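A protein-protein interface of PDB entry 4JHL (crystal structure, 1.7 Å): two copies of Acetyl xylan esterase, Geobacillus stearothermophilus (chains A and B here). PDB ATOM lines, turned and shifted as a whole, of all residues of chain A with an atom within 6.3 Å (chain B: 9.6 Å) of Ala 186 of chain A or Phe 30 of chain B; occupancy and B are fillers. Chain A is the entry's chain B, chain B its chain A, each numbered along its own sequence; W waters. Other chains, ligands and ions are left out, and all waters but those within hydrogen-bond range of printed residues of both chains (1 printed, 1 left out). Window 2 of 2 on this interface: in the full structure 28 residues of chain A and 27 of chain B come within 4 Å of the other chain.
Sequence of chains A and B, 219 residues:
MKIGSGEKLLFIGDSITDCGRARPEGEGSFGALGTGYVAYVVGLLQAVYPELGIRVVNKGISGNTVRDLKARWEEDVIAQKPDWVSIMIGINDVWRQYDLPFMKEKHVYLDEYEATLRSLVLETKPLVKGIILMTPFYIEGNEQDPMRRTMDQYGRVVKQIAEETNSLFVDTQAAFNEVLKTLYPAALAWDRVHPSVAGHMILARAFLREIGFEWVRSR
Leu 183 of chain A touches Gln 46 of chain B.
Ala 186 of chain A touches Phe 30 of chain B (O to CZ, 3.4 Å).
Ala 187 of chain A touches Phe 30 of chain B (O to CZ, 3.96 Å).
Leu 188 of chain A touches Gln 46 of chain B.
Ser 196 of chain A touches Ser 29 of chain B (CB to O, 3.6 Å).
No position is printed for both chains.
Of the 5 pairs that touch across the chains among the printed residues, none has its exchanged pair printed and touching as well.
Of the 17 printed residues of chain B, 3 touch a printed residue of chain A.
Printed residues of chain B that touch a printed residue of chain A: Ser 29, Phe 30 and Gln 46.
Hydrophobic or aromatic side chains of chain B within 4 Å of the printed part of chain A: Phe 30.
Printed residues of chain A that touch a printed residue of chain B: Leu 183, Ala 186, Ala 187, Leu 188 and Ser 196.
Hydrophobic or aromatic side chains of chain A that line the printed part of chain B: Leu 183 and Leu 188.
Among the printed residues, no Asp or Glu carboxylate lies within 4 Å of a Lys or Arg side-chain nitrogen of the other chain.
Water W1 lies within hydrogen-bond range of OG of Ser 29 of chain B and O of Ala 187 of chain A.
Of chain B, only Phe 30 comes within 4 Å of Ala 186 of chain A.
Of the printed residues of chain A, Phe 30 of chain B touches Ala 186 and Ala 187.
No residue of chain B comes within 4 Å of Pro 185 of chain A.
Ala 187 of chain A touches just one residue of chain B: Phe 30.
Printed residues of chain A within 4 Å of Gln 46 of chain B: Leu 183 and Leu 188.
Printed residues of chain B within 4 Å of Leu 188 of chain A: Gln 46 (3.9 Å).
Of the printed residues of chain B, Ser 196 of chain A touches Ser 29 (3.6 Å).
Of the printed residues of chain A, Ser 29 of chain B touches Ser 196 (3.6 Å).
Gly 20 of chain B touches none of the printed residues of chain A.
O of Leu 188 of chain A is in hydrogen-bond range of N of Ser 196 of chain A.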
ATOM      1  N   ILE A 139      -8.391 -16.427 -37.584  1.00  0.00           N
ATOM      2  CA  ILE A 139      -8.919 -17.753 -37.264  1.00  0.00           C
ATOM      3  C   ILE A 139     -10.281 -17.770 -37.880  1.00  0.00           C
ATOM      4  O   ILE A 139     -11.333 -17.434 -37.316  1.00  0.00           O
ATOM      5  CB  ILE A 139      -8.941 -17.983 -35.742  1.00  0.00           C
ATOM      6  CG1 ILE A 139      -7.518 -17.821 -35.177  1.00  0.00           C
ATOM      7  CG2 ILE A 139      -9.525 -19.386 -35.463  1.00  0.00           C
ATOM      8  CD1 ILE A 139      -7.411 -17.850 -33.684  1.00  0.00           C
ATOM      9  N   LEU A 183     -12.828 -27.540 -36.173  1.00  0.00           N
ATOM     10  CA  LEU A 183     -13.425 -26.568 -35.262  1.00  0.00           C
ATOM     11  C   LEU A 183     -13.925 -25.319 -35.978  1.00  0.00           C
ATOM     12  O   LEU A 183     -13.246 -24.811 -36.826  1.00  0.00           O
ATOM     13  CB  LEU A 183     -12.398 -26.183 -34.191  1.00  0.00           C
ATOM     14  CG  LEU A 183     -11.930 -27.307 -33.270  1.00  0.00           C
ATOM     15  CD1 LEU A 183     -10.883 -26.670 -32.400  1.00  0.00           C
ATOM     16  CD2 LEU A 183     -13.001 -27.976 -32.484  1.00  0.00           C
ATOM     17  N   TYR A 184     -15.076 -24.847 -35.561  1.00  0.00           N
ATOM     18  CA  TYR A 184     -15.575 -23.503 -35.925  1.00  0.00           C
ATOM     19  C   TYR A 184     -14.675 -22.490 -35.165  1.00  0.00           C
ATOM     20  O   TYR A 184     -14.237 -22.794 -34.056  1.00  0.00           O
ATOM     21  CB  TYR A 184     -17.026 -23.364 -35.524  1.00  0.00           C
ATOM     22  CG  TYR A 184     -17.675 -22.075 -35.951  1.00  0.00           C
ATOM     23  CD1 TYR A 184     -18.111 -21.897 -37.292  1.00  0.00           C
ATOM     24  CD2 TYR A 184     -17.818 -21.001 -35.070  1.00  0.00           C
ATOM     25  CE1 TYR A 184     -18.650 -20.689 -37.721  1.00  0.00           C
ATOM     26  CE2 TYR A 184     -18.345 -19.799 -35.486  1.00  0.00           C
ATOM     27  CZ  TYR A 184     -18.772 -19.653 -36.825  1.00  0.00           C
ATOM     28  OH  TYR A 184     -19.312 -18.428 -37.234  1.00  0.00           O
ATOM     29  N   PRO A 185     -14.436 -21.311 -35.757  1.00  0.00           N
ATOM     30  CA  PRO A 185     -13.498 -20.357 -35.130  1.00  0.00           C
ATOM     31  C   PRO A 185     -13.767 -20.067 -33.676  1.00  0.00           C
ATOM     32  O   PRO A 185     -12.809 -19.960 -32.891  1.00  0.00           O
ATOM     33  CB  PRO A 185     -13.580 -19.138 -36.007  1.00  0.00           C
ATOM     34  CG  PRO A 185     -13.835 -19.680 -37.364  1.00  0.00           C
ATOM     35  CD  PRO A 185     -14.807 -20.840 -37.120  1.00  0.00           C
ATOM     36  N   ALA A 186     -15.000 -19.916 -33.332  1.00  0.00           N
ATOM     37  CA  ALA A 186     -15.385 -19.533 -32.022  1.00  0.00           C
ATOM     38  C   ALA A 186     -14.903 -20.518 -30.952  1.00  0.00           C
ATOM     39  O   ALA A 186     -14.785 -20.134 -29.814  1.00  0.00           O
ATOM     40  CB  ALA A 186     -16.855 -19.398 -31.826  1.00  0.00           C
ATOM     41  N   ALA A 187     -14.659 -21.778 -31.286  1.00  0.00           N
ATOM     42  CA  ALA A 187     -14.077 -22.729 -30.351  1.00  0.00           C
ATOM     43  C   ALA A 187     -12.633 -22.411 -29.992  1.00  0.00           C
ATOM     44  O   ALA A 187     -12.176 -22.977 -28.997  1.00  0.00           O
ATOM     45  CB  ALA A 187     -14.146 -24.140 -30.877  1.00  0.00           C
ATOM     46  N   LEU A 188     -11.950 -21.643 -30.845  1.00  0.00           N
ATOM     47  CA  LEU A 188     -10.577 -21.208 -30.593  1.00  0.00           C
ATOM     48  C   LEU A 188     -10.529 -19.768 -30.143  1.00  0.00           C
ATOM     49  O   LEU A 188      -9.674 -19.413 -29.363  1.00  0.00           O
ATOM     50  CB  LEU A 188      -9.750 -21.374 -31.833  1.00  0.00           C
ATOM     51  CG  LEU A 188      -9.439 -22.808 -32.227  1.00  0.00           C
ATOM     52  CD1 LEU A 188      -8.873 -22.839 -33.593  1.00  0.00           C
ATOM     53  CD2 LEU A 188      -8.392 -23.420 -31.316  1.00  0.00           C
ATOM     54  N   ALA A 189     -11.365 -18.914 -30.757  1.00  0.00           N
ATOM     55  CA  ALA A 189     -11.352 -17.467 -30.480  1.00  0.00           C
ATOM     56  C   ALA A 189     -12.674 -16.831 -30.859  1.00  0.00           C
ATOM     57  O   ALA A 189     -13.004 -16.734 -32.038  1.00  0.00           O
ATOM     58  CB  ALA A 189     -10.243 -16.764 -31.303  1.00  0.00           C
ATOM     59  N   TRP A 190     -13.407 -16.346 -29.890  1.00  0.00           N
ATOM     60  CA  TRP A 190     -14.629 -15.584 -30.199  1.00  0.00           C
ATOM     61  C   TRP A 190     -14.392 -14.491 -31.208  1.00  0.00           C
ATOM     62  O   TRP A 190     -15.210 -14.316 -32.115  1.00  0.00           O
ATOM     63  CB  TRP A 190     -15.252 -14.994 -28.971  1.00  0.00           C
ATOM     64  CG  TRP A 190     -16.113 -15.877 -28.156  1.00  0.00           C
ATOM     65  CD1 TRP A 190     -16.271 -17.243 -28.239  1.00  0.00           C
ATOM     66  CD2 TRP A 190     -16.936 -15.468 -27.053  1.00  0.00           C
ATOM     67  NE1 TRP A 190     -17.207 -17.663 -27.321  1.00  0.00           N
ATOM     68  CE2 TRP A 190     -17.631 -16.595 -26.598  1.00  0.00           C
ATOM     69  CE3 TRP A 190     -17.182 -14.234 -26.460  1.00  0.00           C
ATOM     70  CZ2 TRP A 190     -18.559 -16.527 -25.521  1.00  0.00           C
ATOM     71  CZ3 TRP A 190     -18.084 -14.144 -25.422  1.00  0.00           C
ATOM     72  CH2 TRP A 190     -18.775 -15.300 -24.966  1.00  0.00           C
ATOM     73  N   ASP A 191     -13.275 -13.763 -31.076  1.00  0.00           N
ATOM     74  CA  ASP A 191     -12.988 -12.645 -31.943  1.00  0.00           C
ATOM     75  C   ASP A 191     -12.210 -12.931 -33.178  1.00  0.00           C
ATOM     76  O   ASP A 191     -11.823 -12.048 -33.930  1.00  0.00           O
ATOM     77  CB  ASP A 191     -12.426 -11.456 -31.162  1.00  0.00           C
ATOM     78  CG  ASP A 191     -11.032 -11.666 -30.631  1.00  0.00           C
ATOM     79  OD1 ASP A 191     -10.383 -12.675 -31.001  1.00  0.00           O
ATOM     80  OD2 ASP A 191     -10.558 -10.858 -29.756  1.00  0.00           O
ATOM     81  N   ARG A 192     -11.907 -14.201 -33.350  1.00  0.00           N
ATOM     82  CA  ARG A 192     -11.089 -14.763 -34.438  1.00  0.00           C
ATOM     83  C   ARG A 192      -9.620 -14.345 -34.471  1.00  0.00           C
ATOM     84  O   ARG A 192      -8.877 -14.600 -35.453  1.00  0.00           O
ATOM     85  CB  ARG A 192     -11.785 -14.568 -35.806  1.00  0.00           C
ATOM     86  CG  ARG A 192     -13.066 -15.305 -35.865  1.00  0.00           C
ATOM     87  CD  ARG A 192     -13.776 -15.110 -37.231  1.00  0.00           C
ATOM     88  NE  ARG A 192     -14.518 -13.851 -37.299  1.00  0.00           N
ATOM     89  CZ  ARG A 192     -15.044 -13.332 -38.401  1.00  0.00           C
ATOM     90  NH1 ARG A 192     -14.981 -13.979 -39.561  1.00  0.00           N
ATOM     91  NH2 ARG A 192     -15.644 -12.152 -38.331  1.00  0.00           N
ATOM     92  N   SER A 196      -7.598 -19.293 -27.304  1.00  0.00           N
ATOM     93  CA  SER A 196      -7.432 -20.104 -26.100  1.00  0.00           C
ATOM     94  C   SER A 196      -5.992 -20.584 -25.976  1.00  0.00           C
ATOM     95  O   SER A 196      -5.148 -20.378 -26.878  1.00  0.00           O
ATOM     96  CB  SER A 196      -8.272 -21.380 -26.199  1.00  0.00           C
ATOM     97  OG  SER A 196      -7.965 -22.053 -27.334  1.00  0.00           O
ATOM     98  N   GLY B  20      -5.837 -22.617 -10.233  1.00  0.00           N
ATOM     99  CA  GLY B  20      -6.884 -21.638 -10.419  1.00  0.00           C
ATOM    100  C   GLY B  20      -8.033 -21.976 -11.310  1.00  0.00           C
ATOM    101  O   GLY B  20      -8.671 -21.082 -11.942  1.00  0.00           O
ATOM    102  N   ARG B  21      -8.360 -23.246 -11.400  1.00  0.00           N
ATOM    103  CA  ARG B  21      -9.506 -23.707 -12.238  1.00  0.00           C
ATOM    104  C   ARG B  21     -10.818 -23.180 -11.685  1.00  0.00           C
ATOM    105  O   ARG B  21     -10.918 -22.784 -10.533  1.00  0.00           O
ATOM    106  CB  ARG B  21      -9.432 -25.220 -12.385  1.00  0.00           C
ATOM    107  CG  ARG B  21      -9.681 -26.009 -11.120  1.00  0.00           C
ATOM    108  CD  ARG B  21     -11.081 -26.165 -10.707  1.00  0.00           C
ATOM    109  NE  ARG B  21     -11.177 -27.090  -9.597  1.00  0.00           N
ATOM    110  CZ  ARG B  21     -12.313 -27.589  -9.167  1.00  0.00           C
ATOM    111  NH1 ARG B  21     -13.500 -27.236  -9.747  1.00  0.00           N
ATOM    112  NH2 ARG B  21     -12.302 -28.445  -8.214  1.00  0.00           N
ATOM    113  N   ALA B  22     -11.846 -23.121 -12.539  1.00  0.00           N
ATOM    114  CA  ALA B  22     -13.211 -22.643 -12.099  1.00  0.00           C
ATOM    115  C   ALA B  22     -13.882 -23.598 -11.198  1.00  0.00           C
ATOM    116  O   ALA B  22     -13.916 -24.783 -11.492  1.00  0.00           O
ATOM    117  CB  ALA B  22     -14.071 -22.518 -13.363  1.00  0.00           C
ATOM    118  N   GLY B  26     -15.134 -26.708 -13.181  1.00  0.00           N
ATOM    119  CA  GLY B  26     -13.859 -27.025 -13.767  1.00  0.00           C
ATOM    120  C   GLY B  26     -13.823 -27.442 -15.214  1.00  0.00           C
ATOM    121  O   GLY B  26     -12.953 -28.149 -15.617  1.00  0.00           O
ATOM    122  N   GLU B  27     -14.703 -26.874 -16.052  1.00  0.00           N
ATOM    123  CA  GLU B  27     -14.750 -27.426 -17.431  1.00  0.00           C
ATOM    124  C   GLU B  27     -14.968 -26.384 -18.463  1.00  0.00           C
ATOM    125  O   GLU B  27     -15.842 -25.565 -18.265  1.00  0.00           O
ATOM    126  CB  GLU B  27     -15.897 -28.475 -17.623  1.00  0.00           C
ATOM    127  CG  GLU B  27     -15.699 -29.206 -18.984  1.00  0.00           C
ATOM    128  CD  GLU B  27     -16.592 -30.428 -19.268  1.00  0.00           C
ATOM    129  OE1 GLU B  27     -17.459 -30.737 -18.422  1.00  0.00           O
ATOM    130  OE2 GLU B  27     -16.375 -31.056 -20.349  1.00  0.00           O
ATOM    131  N   GLY B  28     -14.238 -26.491 -19.598  1.00  0.00           N
ATOM    132  CA  GLY B  28     -14.385 -25.478 -20.643  1.00  0.00           C
ATOM    133  C   GLY B  28     -13.064 -24.990 -21.182  1.00  0.00           C
ATOM    134  O   GLY B  28     -12.028 -25.181 -20.601  1.00  0.00           O
ATOM    135  N   SER B  29     -13.123 -24.357 -22.324  1.00  0.00           N
ATOM    136  CA  SER B  29     -11.950 -24.156 -23.174  1.00  0.00           C
ATOM    137  C   SER B  29     -11.219 -22.820 -22.873  1.00  0.00           C
ATOM    138  O   SER B  29     -10.098 -22.626 -23.369  1.00  0.00           O
ATOM    139  CB  SER B  29     -12.435 -24.128 -24.650  1.00  0.00           C
ATOM    140  OG  SER B  29     -12.648 -25.471 -25.086  1.00  0.00           O
ATOM    141  N   PHE B  30     -11.905 -21.947 -22.104  1.00  0.00           N
ATOM    142  CA  PHE B  30     -11.641 -20.484 -22.106  1.00  0.00           C
ATOM    143  C   PHE B  30     -11.092 -19.962 -20.725  1.00  0.00           C
ATOM    144  O   PHE B  30     -11.214 -18.769 -20.401  1.00  0.00           O
ATOM    145  CB  PHE B  30     -12.918 -19.698 -22.532  1.00  0.00           C
ATOM    146  CG  PHE B  30     -13.452 -20.092 -23.959  1.00  0.00           C
ATOM    147  CD1 PHE B  30     -12.899 -19.519 -25.119  1.00  0.00           C
ATOM    148  CD2 PHE B  30     -14.529 -20.991 -24.119  1.00  0.00           C
ATOM    149  CE1 PHE B  30     -13.377 -19.889 -26.440  1.00  0.00           C
ATOM    150  CE2 PHE B  30     -15.001 -21.355 -25.416  1.00  0.00           C
ATOM    151  CZ  PHE B  30     -14.410 -20.820 -26.545  1.00  0.00           C
ATOM    152  N   GLY B  31     -10.548 -20.861 -19.906  1.00  0.00           N
ATOM    153  CA  GLY B  31      -9.899 -20.477 -18.655  1.00  0.00           C
ATOM    154  C   GLY B  31     -10.353 -21.298 -17.439  1.00  0.00           C
ATOM    155  O   GLY B  31      -9.706 -21.350 -16.372  1.00  0.00           O
ATOM    156  N   ALA B  32     -11.441 -22.018 -17.591  1.00  0.00           N
ATOM    157  CA  ALA B  32     -12.009 -22.866 -16.535  1.00  0.00           C
ATOM    158  C   ALA B  32     -11.016 -23.992 -16.046  1.00  0.00           C
ATOM    159  O   ALA B  32     -11.134 -24.540 -14.977  1.00  0.00           O
ATOM    160  CB  ALA B  32     -13.233 -23.527 -17.058  1.00  0.00           C
ATOM    161  N   LEU B  33     -10.129 -24.347 -16.922  1.00  0.00           N
ATOM    162  CA  LEU B  33      -9.163 -25.436 -16.652  1.00  0.00           C
ATOM    163  C   LEU B  33      -7.973 -24.987 -15.800  1.00  0.00           C
ATOM    164  O   LEU B  33      -7.115 -25.825 -15.465  1.00  0.00           O
ATOM    165  CB  LEU B  33      -8.696 -26.078 -17.933  1.00  0.00           C
ATOM    166  CG  LEU B  33      -9.797 -26.809 -18.719  1.00  0.00           C
ATOM    167  CD1 LEU B  33      -9.186 -27.216 -20.045  1.00  0.00           C
ATOM    168  CD2 LEU B  33     -10.310 -28.004 -17.940  1.00  0.00           C
ATOM    169  N   GLY B  34      -7.834 -23.694 -15.574  1.00  0.00           N
ATOM    170  CA  GLY B  34      -6.648 -23.156 -14.882  1.00  0.00           C
ATOM    171  C   GLY B  34      -5.516 -22.942 -15.764  1.00  0.00           C
ATOM    172  O   GLY B  34      -5.633 -23.025 -16.959  1.00  0.00           O
ATOM    173  N   THR B  35      -4.333 -22.669 -15.204  1.00  0.00           N
ATOM    174  CA  THR B  35      -3.212 -22.194 -15.952  1.00  0.00           C
ATOM    175  C   THR B  35      -1.937 -23.049 -15.905  1.00  0.00           C
ATOM    176  O   THR B  35      -0.827 -22.571 -16.138  1.00  0.00           O
ATOM    177  CB  THR B  35      -2.838 -20.762 -15.476  1.00  0.00           C
ATOM    178  OG1 THR B  35      -2.528 -20.772 -14.102  1.00  0.00           O
ATOM    179  CG2 THR B  35      -3.968 -19.838 -15.699  1.00  0.00           C
ATOM    180  N   ALA B  39      -4.399 -27.544 -18.351  1.00  0.00           N
ATOM    181  CA  ALA B  39      -4.676 -26.699 -19.513  1.00  0.00           C
ATOM    182  C   ALA B  39      -3.733 -26.954 -20.650  1.00  0.00           C
ATOM    183  O   ALA B  39      -4.163 -26.938 -21.809  1.00  0.00           O
ATOM    184  CB  ALA B  39      -4.645 -25.261 -19.078  1.00  0.00           C
ATOM    185  N   VAL B  42      -4.750 -30.117 -22.458  1.00  0.00           N
ATOM    186  CA  VAL B  42      -5.939 -29.932 -23.249  1.00  0.00           C
ATOM    187  C   VAL B  42      -5.580 -29.123 -24.483  1.00  0.00           C
ATOM    188  O   VAL B  42      -6.104 -29.403 -25.605  1.00  0.00           O
ATOM    189  CB  VAL B  42      -7.041 -29.296 -22.416  1.00  0.00           C
ATOM    190  CG1 VAL B  42      -8.256 -29.024 -23.271  1.00  0.00           C
ATOM    191  CG2 VAL B  42      -7.508 -30.247 -21.346  1.00  0.00           C
ATOM    192  N   GLN B  46      -5.915 -30.521 -28.351  1.00  0.00           N
ATOM    193  CA  GLN B  46      -6.703 -29.754 -29.282  1.00  0.00           C
ATOM    194  C   GLN B  46      -5.880 -29.330 -30.490  1.00  0.00           C
ATOM    195  O   GLN B  46      -6.404 -29.329 -31.640  1.00  0.00           O
ATOM    196  CB  GLN B  46      -7.487 -28.620 -28.655  1.00  0.00           C
ATOM    197  CG  GLN B  46      -8.426 -28.051 -29.700  1.00  0.00           C
ATOM    198  CD  GLN B  46      -9.522 -27.228 -29.057  1.00  0.00           C
ATOM    199  OE1 GLN B  46      -9.283 -26.107 -28.637  1.00  0.00           O
ATOM    200  NE2 GLN B  46     -10.726 -27.798 -28.949  1.00  0.00           N
ATOM    201  N   VAL B  56     -12.788 -32.293 -21.050  1.00  0.00           N
ATOM    202  CA  VAL B  56     -11.796 -32.382 -19.984  1.00  0.00           C
ATOM    203  C   VAL B  56     -12.315 -31.554 -18.841  1.00  0.00           C
ATOM    204  O   VAL B  56     -12.830 -30.456 -19.011  1.00  0.00           O
ATOM    205  CB  VAL B  56     -10.388 -31.921 -20.385  1.00  0.00           C
ATOM    206  CG1 VAL B  56      -9.442 -32.004 -19.133  1.00  0.00           C
ATOM    207  CG2 VAL B  56      -9.809 -32.804 -21.476  1.00  0.00           C
HETATM  208  O   HOH W   1     -13.695 -24.600 -27.350  1.00  0.00           O
